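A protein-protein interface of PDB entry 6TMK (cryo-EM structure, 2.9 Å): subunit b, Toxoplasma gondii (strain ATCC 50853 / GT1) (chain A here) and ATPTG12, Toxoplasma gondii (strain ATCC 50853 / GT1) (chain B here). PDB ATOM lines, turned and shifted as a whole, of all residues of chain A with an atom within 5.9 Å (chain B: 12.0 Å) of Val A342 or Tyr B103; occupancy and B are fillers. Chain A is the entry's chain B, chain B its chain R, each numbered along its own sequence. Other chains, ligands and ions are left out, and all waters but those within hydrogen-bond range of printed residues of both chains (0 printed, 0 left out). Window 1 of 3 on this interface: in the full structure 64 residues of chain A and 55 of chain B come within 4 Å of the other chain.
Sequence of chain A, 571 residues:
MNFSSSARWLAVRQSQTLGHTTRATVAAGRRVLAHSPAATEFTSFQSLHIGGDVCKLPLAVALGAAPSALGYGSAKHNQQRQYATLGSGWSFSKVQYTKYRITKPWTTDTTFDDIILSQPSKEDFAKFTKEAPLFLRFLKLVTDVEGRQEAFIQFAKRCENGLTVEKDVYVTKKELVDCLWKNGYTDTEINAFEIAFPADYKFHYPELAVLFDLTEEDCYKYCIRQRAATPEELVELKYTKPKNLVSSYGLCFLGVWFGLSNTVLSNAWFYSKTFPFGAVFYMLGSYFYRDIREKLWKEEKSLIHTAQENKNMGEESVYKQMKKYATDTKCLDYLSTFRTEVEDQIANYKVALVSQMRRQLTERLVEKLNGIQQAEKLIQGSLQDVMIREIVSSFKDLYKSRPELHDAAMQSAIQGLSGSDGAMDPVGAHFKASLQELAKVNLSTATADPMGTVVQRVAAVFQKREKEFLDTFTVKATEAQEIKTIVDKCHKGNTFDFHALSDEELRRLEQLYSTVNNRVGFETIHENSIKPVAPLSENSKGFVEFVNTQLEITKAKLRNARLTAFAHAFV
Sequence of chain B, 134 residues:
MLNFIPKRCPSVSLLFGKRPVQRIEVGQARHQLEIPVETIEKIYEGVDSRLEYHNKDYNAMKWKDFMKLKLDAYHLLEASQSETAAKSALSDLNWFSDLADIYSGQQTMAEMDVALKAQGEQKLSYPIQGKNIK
The side-chain amide oxygen (OE1) of Gln A345 lies within hydrogen-bond range of the side-chain hydroxyl (OH) of Tyr B103 (2.7 Å).
Among the printed residues, merely in contact across the chains: Val A342 with Tyr B103 and Ile A346 with Ala B110.
No residue of chain B comes within 4 Å of Thr A340.
No residue of chain B comes within 4 Å of Glu A341.
Printed residues of chain B within 4 Å of Val A342: Tyr B103.
No residue of chain B comes within 4 Å of Glu A343.
Ile A346 touches just one residue of chain B: Ala B110.
Leu B99 touches none of the printed residues of chain A.
Of the printed residues of chain A, Ala B110 touches Ile A346 (3.7 Å).
Glu B111 touches none of the printed residues of chain A.
The nearest residue of chain B that does not touch Val A342 is Gln B106 (4.7 Å).
The nearest residue of chain A that does not touch Tyr B103 is Phe A338 (4.3 Å).
The nearest printed residue of chain A that does not touch Ala B110 is Ala A347 (6.6 Å).
Of the 11 printed residues of chain A, 3 touch a printed residue of chain B.
Printed residues of chain A that touch a printed residue of chain B: Val A342, Gln A345 and Ile A346.
Of the 18 printed residues of chain B, 2 touch a printed residue of chain A.
Printed residues of chain B that touch a printed residue of chain A: Tyr B103 and Ala B110.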
ATOM      1  N   THR A 337       0.015 -13.910 -20.011  1.00  0.00           N
ATOM      2  CA  THR A 337      -1.152 -14.554 -19.414  1.00  0.00           C
ATOM      3  C   THR A 337      -1.672 -13.759 -18.224  1.00  0.00           C
ATOM      4  O   THR A 337      -2.876 -13.778 -17.942  1.00  0.00           O
ATOM      5  CB  THR A 337      -0.816 -15.983 -18.983  1.00  0.00           C
ATOM      6  OG1 THR A 337      -0.125 -15.958 -17.729  1.00  0.00           O
ATOM      7  CG2 THR A 337       0.040 -16.682 -20.030  1.00  0.00           C
ATOM      8  N   PHE A 338      -0.776 -13.075 -17.513  1.00  0.00           N
ATOM      9  CA  PHE A 338      -1.123 -12.401 -16.265  1.00  0.00           C
ATOM     10  C   PHE A 338      -2.411 -11.595 -16.392  1.00  0.00           C
ATOM     11  O   PHE A 338      -3.337 -11.751 -15.588  1.00  0.00           O
ATOM     12  CB  PHE A 338       0.040 -11.501 -15.851  1.00  0.00           C
ATOM     13  CG  PHE A 338      -0.050 -10.993 -14.447  1.00  0.00           C
ATOM     14  CD1 PHE A 338       0.332 -11.789 -13.384  1.00  0.00           C
ATOM     15  CD2 PHE A 338      -0.486  -9.708 -14.192  1.00  0.00           C
ATOM     16  CE1 PHE A 338       0.261 -11.320 -12.091  1.00  0.00           C
ATOM     17  CE2 PHE A 338      -0.558  -9.231 -12.902  1.00  0.00           C
ATOM     18  CZ  PHE A 338      -0.184 -10.038 -11.849  1.00  0.00           C
ATOM     19  N   ARG A 339      -2.493 -10.726 -17.401  1.00  0.00           N
ATOM     20  CA  ARG A 339      -3.692  -9.913 -17.576  1.00  0.00           C
ATOM     21  C   ARG A 339      -4.914 -10.766 -17.885  1.00  0.00           C
ATOM     22  O   ARG A 339      -6.027 -10.431 -17.463  1.00  0.00           O
ATOM     23  CB  ARG A 339      -3.468  -8.893 -18.693  1.00  0.00           C
ATOM     24  CG  ARG A 339      -4.704  -8.096 -19.087  1.00  0.00           C
ATOM     25  CD  ARG A 339      -5.259  -7.305 -17.918  1.00  0.00           C
ATOM     26  NE  ARG A 339      -6.394  -6.475 -18.311  1.00  0.00           N
ATOM     27  CZ  ARG A 339      -6.298  -5.385 -19.066  1.00  0.00           C
ATOM     28  NH1 ARG A 339      -7.385  -4.690 -19.369  1.00  0.00           N
ATOM     29  NH2 ARG A 339      -5.118  -4.980 -19.510  1.00  0.00           N
ATOM     30  N   THR A 340      -4.732 -11.866 -18.613  1.00  0.00           N
ATOM     31  CA  THR A 340      -5.861 -12.720 -18.965  1.00  0.00           C
ATOM     32  C   THR A 340      -6.386 -13.487 -17.756  1.00  0.00           C
ATOM     33  O   THR A 340      -7.595 -13.713 -17.636  1.00  0.00           O
ATOM     34  CB  THR A 340      -5.454 -13.691 -20.071  1.00  0.00           C
ATOM     35  OG1 THR A 340      -5.212 -12.966 -21.283  1.00  0.00           O
ATOM     36  CG2 THR A 340      -6.544 -14.723 -20.306  1.00  0.00           C
ATOM     37  N   GLU A 341      -5.495 -13.898 -16.854  1.00  0.00           N
ATOM     38  CA  GLU A 341      -5.899 -14.742 -15.734  1.00  0.00           C
ATOM     39  C   GLU A 341      -6.555 -13.935 -14.618  1.00  0.00           C
ATOM     40  O   GLU A 341      -7.649 -14.278 -14.160  1.00  0.00           O
ATOM     41  CB  GLU A 341      -4.688 -15.504 -15.198  1.00  0.00           C
ATOM     42  CG  GLU A 341      -4.296 -16.694 -16.051  1.00  0.00           C
ATOM     43  CD  GLU A 341      -3.172 -17.506 -15.440  1.00  0.00           C
ATOM     44  OE1 GLU A 341      -3.064 -17.533 -14.197  1.00  0.00           O
ATOM     45  OE2 GLU A 341      -2.395 -18.116 -16.204  1.00  0.00           O
ATOM     46  N   VAL A 342      -5.889 -12.880 -14.149  1.00  0.00           N
ATOM     47  CA  VAL A 342      -6.343 -12.186 -12.946  1.00  0.00           C
ATOM     48  C   VAL A 342      -7.718 -11.561 -13.150  1.00  0.00           C
ATOM     49  O   VAL A 342      -8.521 -11.488 -12.206  1.00  0.00           O
ATOM     50  CB  VAL A 342      -5.297 -11.132 -12.537  1.00  0.00           C
ATOM     51  CG1 VAL A 342      -5.916 -10.065 -11.651  1.00  0.00           C
ATOM     52  CG2 VAL A 342      -4.134 -11.800 -11.838  1.00  0.00           C
ATOM     53  N   GLU A 343      -8.069 -11.245 -14.397  1.00  0.00           N
ATOM     54  CA  GLU A 343      -9.390 -10.741 -14.750  1.00  0.00           C
ATOM     55  C   GLU A 343     -10.432 -11.841 -14.850  1.00  0.00           C
ATOM     56  O   GLU A 343     -11.531 -11.605 -15.364  1.00  0.00           O
ATOM     57  CB  GLU A 343      -9.316  -9.981 -16.077  1.00  0.00           C
ATOM     58  CG  GLU A 343      -8.529  -8.684 -16.000  1.00  0.00           C
ATOM     59  CD  GLU A 343      -9.404  -7.485 -15.702  1.00  0.00           C
ATOM     60  OE1 GLU A 343     -10.507  -7.675 -15.147  1.00  0.00           O
ATOM     61  OE2 GLU A 343      -8.988  -6.350 -16.020  1.00  0.00           O
ATOM     62  N   ASP A 344     -10.105 -13.015 -14.377  1.00  0.00           N
ATOM     63  CA  ASP A 344     -10.999 -14.151 -14.218  1.00  0.00           C
ATOM     64  C   ASP A 344     -10.938 -14.684 -12.799  1.00  0.00           C
ATOM     65  O   ASP A 344     -11.969 -15.044 -12.232  1.00  0.00           O
ATOM     66  CB  ASP A 344     -10.635 -15.255 -15.214  1.00  0.00           C
ATOM     67  CG  ASP A 344     -11.772 -16.226 -15.449  1.00  0.00           C
ATOM     68  OD1 ASP A 344     -12.732 -15.857 -16.156  1.00  0.00           O
ATOM     69  OD2 ASP A 344     -11.705 -17.358 -14.926  1.00  0.00           O
ATOM     70  N   GLN A 345      -9.737 -14.769 -12.229  1.00  0.00           N
ATOM     71  CA  GLN A 345      -9.564 -15.079 -10.814  1.00  0.00           C
ATOM     72  C   GLN A 345     -10.231 -14.049  -9.903  1.00  0.00           C
ATOM     73  O   GLN A 345     -10.701 -14.408  -8.817  1.00  0.00           O
ATOM     74  CB  GLN A 345      -8.074 -15.183 -10.490  1.00  0.00           C
ATOM     75  CG  GLN A 345      -7.754 -15.217  -9.003  1.00  0.00           C
ATOM     76  CD  GLN A 345      -6.295 -15.544  -8.690  1.00  0.00           C
ATOM     77  OE1 GLN A 345      -5.873 -15.459  -7.538  1.00  0.00           O
ATOM     78  NE2 GLN A 345      -5.522 -15.918  -9.708  1.00  0.00           N
ATOM     79  N   ILE A 346     -10.479 -12.833 -10.387  1.00  0.00           N
ATOM     80  CA  ILE A 346     -11.200 -11.890  -9.540  1.00  0.00           C
ATOM     81  C   ILE A 346     -12.702 -12.133  -9.628  1.00  0.00           C
ATOM     82  O   ILE A 346     -13.421 -12.045  -8.620  1.00  0.00           O
ATOM     83  CB  ILE A 346     -10.831 -10.449  -9.939  1.00  0.00           C
ATOM     84  CG1 ILE A 346      -9.413 -10.103  -9.476  1.00  0.00           C
ATOM     85  CG2 ILE A 346     -11.831  -9.460  -9.370  1.00  0.00           C
ATOM     86  CD1 ILE A 346      -9.230 -10.062  -7.972  1.00  0.00           C
ATOM     87  N   ALA A 347     -13.207 -12.410 -10.827  1.00  0.00           N
ATOM     88  CA  ALA A 347     -14.617 -12.752 -10.945  1.00  0.00           C
ATOM     89  C   ALA A 347     -14.928 -14.074 -10.252  1.00  0.00           C
ATOM     90  O   ALA A 347     -16.056 -14.271  -9.787  1.00  0.00           O
ATOM     91  CB  ALA A 347     -15.015 -12.816 -12.418  1.00  0.00           C
ATOM     92  N   TRP B  95       9.882  -4.620 -13.013  1.00  0.00           N
ATOM     93  CA  TRP B  95       8.436  -4.517 -13.165  1.00  0.00           C
ATOM     94  C   TRP B  95       7.693  -5.599 -12.386  1.00  0.00           C
ATOM     95  O   TRP B  95       6.602  -6.017 -12.777  1.00  0.00           O
ATOM     96  CB  TRP B  95       8.050  -4.545 -14.644  1.00  0.00           C
ATOM     97  CG  TRP B  95       8.860  -5.476 -15.489  1.00  0.00           C
ATOM     98  CD1 TRP B  95       9.757  -5.127 -16.456  1.00  0.00           C
ATOM     99  CD2 TRP B  95       8.823  -6.907 -15.476  1.00  0.00           C
ATOM    100  NE1 TRP B  95      10.295  -6.250 -17.031  1.00  0.00           N
ATOM    101  CE2 TRP B  95       9.735  -7.357 -16.449  1.00  0.00           C
ATOM    102  CE3 TRP B  95       8.113  -7.851 -14.733  1.00  0.00           C
ATOM    103  CZ2 TRP B  95       9.956  -8.707 -16.696  1.00  0.00           C
ATOM    104  CZ3 TRP B  95       8.335  -9.192 -14.979  1.00  0.00           C
ATOM    105  CH2 TRP B  95       9.248  -9.606 -15.952  1.00  0.00           C
ATOM    106  N   PHE B  96       8.267  -6.054 -11.274  1.00  0.00           N
ATOM    107  CA  PHE B  96       7.549  -6.926 -10.353  1.00  0.00           C
ATOM    108  C   PHE B  96       6.806  -6.127  -9.293  1.00  0.00           C
ATOM    109  O   PHE B  96       5.749  -6.562  -8.811  1.00  0.00           O
ATOM    110  CB  PHE B  96       8.522  -7.887  -9.666  1.00  0.00           C
ATOM    111  CG  PHE B  96       9.096  -8.927 -10.580  1.00  0.00           C
ATOM    112  CD1 PHE B  96       8.278  -9.851 -11.200  1.00  0.00           C
ATOM    113  CD2 PHE B  96      10.458  -8.979 -10.818  1.00  0.00           C
ATOM    114  CE1 PHE B  96       8.806 -10.808 -12.039  1.00  0.00           C
ATOM    115  CE2 PHE B  96      10.989  -9.934 -11.657  1.00  0.00           C
ATOM    116  CZ  PHE B  96      10.162 -10.850 -12.268  1.00  0.00           C
ATOM    117  N   SER B  97       7.285  -4.917  -9.008  1.00  0.00           N
ATOM    118  CA  SER B  97       6.608  -4.051  -8.052  1.00  0.00           C
ATOM    119  C   SER B  97       5.272  -3.593  -8.613  1.00  0.00           C
ATOM    120  O   SER B  97       4.259  -3.587  -7.905  1.00  0.00           O
ATOM    121  CB  SER B  97       7.494  -2.855  -7.712  1.00  0.00           C
ATOM    122  OG  SER B  97       7.580  -1.960  -8.807  1.00  0.00           O
ATOM    123  N   ASP B  98       5.257  -3.172  -9.877  1.00  0.00           N
ATOM    124  CA  ASP B  98       4.017  -2.689 -10.465  1.00  0.00           C
ATOM    125  C   ASP B  98       2.994  -3.814 -10.534  1.00  0.00           C
ATOM    126  O   ASP B  98       1.799  -3.596 -10.309  1.00  0.00           O
ATOM    127  CB  ASP B  98       4.285  -2.116 -11.855  1.00  0.00           C
ATOM    128  CG  ASP B  98       5.430  -1.123 -11.866  1.00  0.00           C
ATOM    129  OD1 ASP B  98       5.817  -0.648 -10.777  1.00  0.00           O
ATOM    130  OD2 ASP B  98       5.945  -0.818 -12.961  1.00  0.00           O
ATOM    131  N   LEU B  99       3.450  -5.031 -10.838  1.00  0.00           N
ATOM    132  CA  LEU B  99       2.548  -6.178 -10.868  1.00  0.00           C
ATOM    133  C   LEU B  99       1.956  -6.440  -9.490  1.00  0.00           C
ATOM    134  O   LEU B  99       0.747  -6.658  -9.352  1.00  0.00           O
ATOM    135  CB  LEU B  99       3.288  -7.412 -11.375  1.00  0.00           C
ATOM    136  CG  LEU B  99       3.202  -7.668 -12.879  1.00  0.00           C
ATOM    137  CD1 LEU B  99       3.440  -6.387 -13.660  1.00  0.00           C
ATOM    138  CD2 LEU B  99       4.198  -8.736 -13.282  1.00  0.00           C
ATOM    139  N   ALA B 100       2.794  -6.407  -8.451  1.00  0.00           N
ATOM    140  CA  ALA B 100       2.279  -6.592  -7.098  1.00  0.00           C
ATOM    141  C   ALA B 100       1.271  -5.506  -6.744  1.00  0.00           C
ATOM    142  O   ALA B 100       0.219  -5.785  -6.150  1.00  0.00           O
ATOM    143  CB  ALA B 100       3.432  -6.600  -6.097  1.00  0.00           C
ATOM    144  N   ASP B 101       1.579  -4.258  -7.100  1.00  0.00           N
ATOM    145  CA  ASP B 101       0.698  -3.147  -6.766  1.00  0.00           C
ATOM    146  C   ASP B 101      -0.648  -3.281  -7.464  1.00  0.00           C
ATOM    147  O   ASP B 101      -1.696  -3.078  -6.843  1.00  0.00           O
ATOM    148  CB  ASP B 101       1.364  -1.823  -7.136  1.00  0.00           C
ATOM    149  CG  ASP B 101       2.599  -1.537  -6.303  1.00  0.00           C
ATOM    150  OD1 ASP B 101       3.480  -0.790  -6.779  1.00  0.00           O
ATOM    151  OD2 ASP B 101       2.689  -2.060  -5.173  1.00  0.00           O
ATOM    152  N   ILE B 102      -0.647  -3.662  -8.744  1.00  0.00           N
ATOM    153  CA  ILE B 102      -1.919  -3.775  -9.451  1.00  0.00           C
ATOM    154  C   ILE B 102      -2.685  -4.994  -8.966  1.00  0.00           C
ATOM    155  O   ILE B 102      -3.921  -4.994  -8.960  1.00  0.00           O
ATOM    156  CB  ILE B 102      -1.711  -3.814 -10.976  1.00  0.00           C
ATOM    157  CG1 ILE B 102      -0.962  -5.083 -11.381  1.00  0.00           C
ATOM    158  CG2 ILE B 102      -0.990  -2.558 -11.445  1.00  0.00           C
ATOM    159  CD1 ILE B 102      -0.676  -5.171 -12.857  1.00  0.00           C
ATOM    160  N   TYR B 103      -1.985  -6.043  -8.535  1.00  0.00           N
ATOM    161  CA  TYR B 103      -2.681  -7.198  -7.981  1.00  0.00           C
ATOM    162  C   TYR B 103      -3.404  -6.817  -6.698  1.00  0.00           C
ATOM    163  O   TYR B 103      -4.598  -7.101  -6.531  1.00  0.00           O
ATOM    164  CB  TYR B 103      -1.700  -8.339  -7.726  1.00  0.00           C
ATOM    165  CG  TYR B 103      -2.375  -9.681  -7.576  1.00  0.00           C
ATOM    166  CD1 TYR B 103      -3.093 -10.238  -8.623  1.00  0.00           C
ATOM    167  CD2 TYR B 103      -2.297 -10.389  -6.387  1.00  0.00           C
ATOM    168  CE1 TYR B 103      -3.713 -11.460  -8.490  1.00  0.00           C
ATOM    169  CE2 TYR B 103      -2.914 -11.616  -6.245  1.00  0.00           C
ATOM    170  CZ  TYR B 103      -3.622 -12.146  -7.300  1.00  0.00           C
ATOM    171  OH  TYR B 103      -4.240 -13.366  -7.171  1.00  0.00           O
ATOM    172  N   SER B 104      -2.686  -6.182  -5.767  1.00  0.00           N
ATOM    173  CA  SER B 104      -3.319  -5.718  -4.537  1.00  0.00           C
ATOM    174  C   SER B 104      -4.452  -4.745  -4.840  1.00  0.00           C
ATOM    175  O   SER B 104      -5.496  -4.767  -4.174  1.00  0.00           O
ATOM    176  CB  SER B 104      -2.279  -5.064  -3.629  1.00  0.00           C
ATOM    177  OG  SER B 104      -1.274  -5.991  -3.258  1.00  0.00           O
ATOM    178  N   GLY B 105      -4.279  -3.908  -5.863  1.00  0.00           N
ATOM    179  CA  GLY B 105      -5.311  -2.945  -6.200  1.00  0.00           C
ATOM    180  C   GLY B 105      -6.571  -3.611  -6.710  1.00  0.00           C
ATOM    181  O   GLY B 105      -7.678  -3.245  -6.312  1.00  0.00           O
ATOM    182  N   GLN B 106      -6.425  -4.601  -7.591  1.00  0.00           N
ATOM    183  CA  GLN B 106      -7.589  -5.314  -8.102  1.00  0.00           C
ATOM    184  C   GLN B 106      -8.264  -6.105  -6.991  1.00  0.00           C
ATOM    185  O   GLN B 106      -9.498  -6.153  -6.911  1.00  0.00           O
ATOM    186  CB  GLN B 106      -7.172  -6.239  -9.242  1.00  0.00           C
ATOM    187  CG  GLN B 106      -6.982  -5.533 -10.572  1.00  0.00           C
ATOM    188  CD  GLN B 106      -8.289  -5.072 -11.179  1.00  0.00           C
ATOM    189  OE1 GLN B 106      -8.499  -3.879 -11.397  1.00  0.00           O
ATOM    190  NE2 GLN B 106      -9.175  -6.019 -11.459  1.00  0.00           N
ATOM    191  N   GLN B 107      -7.467  -6.718  -6.114  1.00  0.00           N
ATOM    192  CA  GLN B 107      -8.023  -7.444  -4.977  1.00  0.00           C
ATOM    193  C   GLN B 107      -8.881  -6.527  -4.114  1.00  0.00           C
ATOM    194  O   GLN B 107     -10.035  -6.845  -3.797  1.00  0.00           O
ATOM    195  CB  GLN B 107      -6.892  -8.058  -4.155  1.00  0.00           C
ATOM    196  CG  GLN B 107      -7.351  -8.786  -2.907  1.00  0.00           C
ATOM    197  CD  GLN B 107      -6.424  -9.924  -2.529  1.00  0.00           C
ATOM    198  OE1 GLN B 107      -6.387 -10.956  -3.198  1.00  0.00           O
ATOM    199  NE2 GLN B 107      -5.666  -9.738  -1.456  1.00  0.00           N
ATOM    200  N   THR B 108      -8.330  -5.375  -3.726  1.00  0.00           N
ATOM    201  CA  THR B 108      -9.072  -4.438  -2.889  1.00  0.00           C
ATOM    202  C   THR B 108     -10.291  -3.884  -3.620  1.00  0.00           C
ATOM    203  O   THR B 108     -11.363  -3.721  -3.022  1.00  0.00           O
ATOM    204  CB  THR B 108      -8.150  -3.304  -2.443  1.00  0.00           C
ATOM    205  OG1 THR B 108      -7.148  -3.817  -1.558  1.00  0.00           O
ATOM    206  CG2 THR B 108      -8.934  -2.218  -1.739  1.00  0.00           C
ATOM    207  N   MET B 109     -10.146  -3.572  -4.909  1.00  0.00           N
ATOM    208  CA  MET B 109     -11.263  -3.021  -5.666  1.00  0.00           C
ATOM    209  C   MET B 109     -12.401  -4.023  -5.777  1.00  0.00           C
ATOM    210  O   MET B 109     -13.570  -3.636  -5.735  1.00  0.00           O
ATOM    211  CB  MET B 109     -10.779  -2.591  -7.053  1.00  0.00           C
ATOM    212  CG  MET B 109     -11.857  -2.516  -8.127  1.00  0.00           C
ATOM    213  SD  MET B 109     -13.170  -1.346  -7.735  1.00  0.00           S
ATOM    214  CE  MET B 109     -14.162  -1.450  -9.223  1.00  0.00           C
ATOM    215  N   ALA B 110     -12.090  -5.317  -5.856  1.00  0.00           N
ATOM    216  CA  ALA B 110     -13.147  -6.322  -5.818  1.00  0.00           C
ATOM    217  C   ALA B 110     -13.757  -6.412  -4.424  1.00  0.00           C
ATOM    218  O   ALA B 110     -14.985  -6.467  -4.267  1.00  0.00           O
ATOM    219  CB  ALA B 110     -12.600  -7.679  -6.256  1.00  0.00           C
ATOM    220  N   GLU B 111     -12.905  -6.445  -3.396  1.00  0.00           N
ATOM    221  CA  GLU B 111     -13.396  -6.568  -2.028  1.00  0.00           C
ATOM    222  C   GLU B 111     -14.346  -5.432  -1.667  1.00  0.00           C
ATOM    223  O   GLU B 111     -15.269  -5.628  -0.867  1.00  0.00           O
ATOM    224  CB  GLU B 111     -12.218  -6.596  -1.055  1.00  0.00           C
ATOM    225  CG  GLU B 111     -11.859  -7.984  -0.556  1.00  0.00           C
ATOM    226  CD  GLU B 111     -10.592  -7.991   0.276  1.00  0.00           C
ATOM    227  OE1 GLU B 111     -10.337  -6.995   0.985  1.00  0.00           O
ATOM    228  OE2 GLU B 111      -9.849  -8.993   0.219  1.00  0.00           O
ATOM    229  N   MET B 112     -14.142  -4.248  -2.242  1.00  0.00           N
ATOM    230  CA  MET B 112     -14.960  -3.080  -1.935  1.00  0.00           C
ATOM    231  C   MET B 112     -15.887  -2.677  -3.080  1.00  0.00           C
ATOM    232  O   MET B 112     -16.555  -1.642  -2.986  1.00  0.00           O
ATOM    233  CB  MET B 112     -14.065  -1.904  -1.537  1.00  0.00           C
ATOM    234  CG  MET B 112     -13.600  -1.033  -2.683  1.00  0.00           C
ATOM    235  SD  MET B 112     -12.199  -0.017  -2.188  1.00  0.00           S
ATOM    236  CE  MET B 112     -12.215   1.217  -3.478  1.00  0.00           C
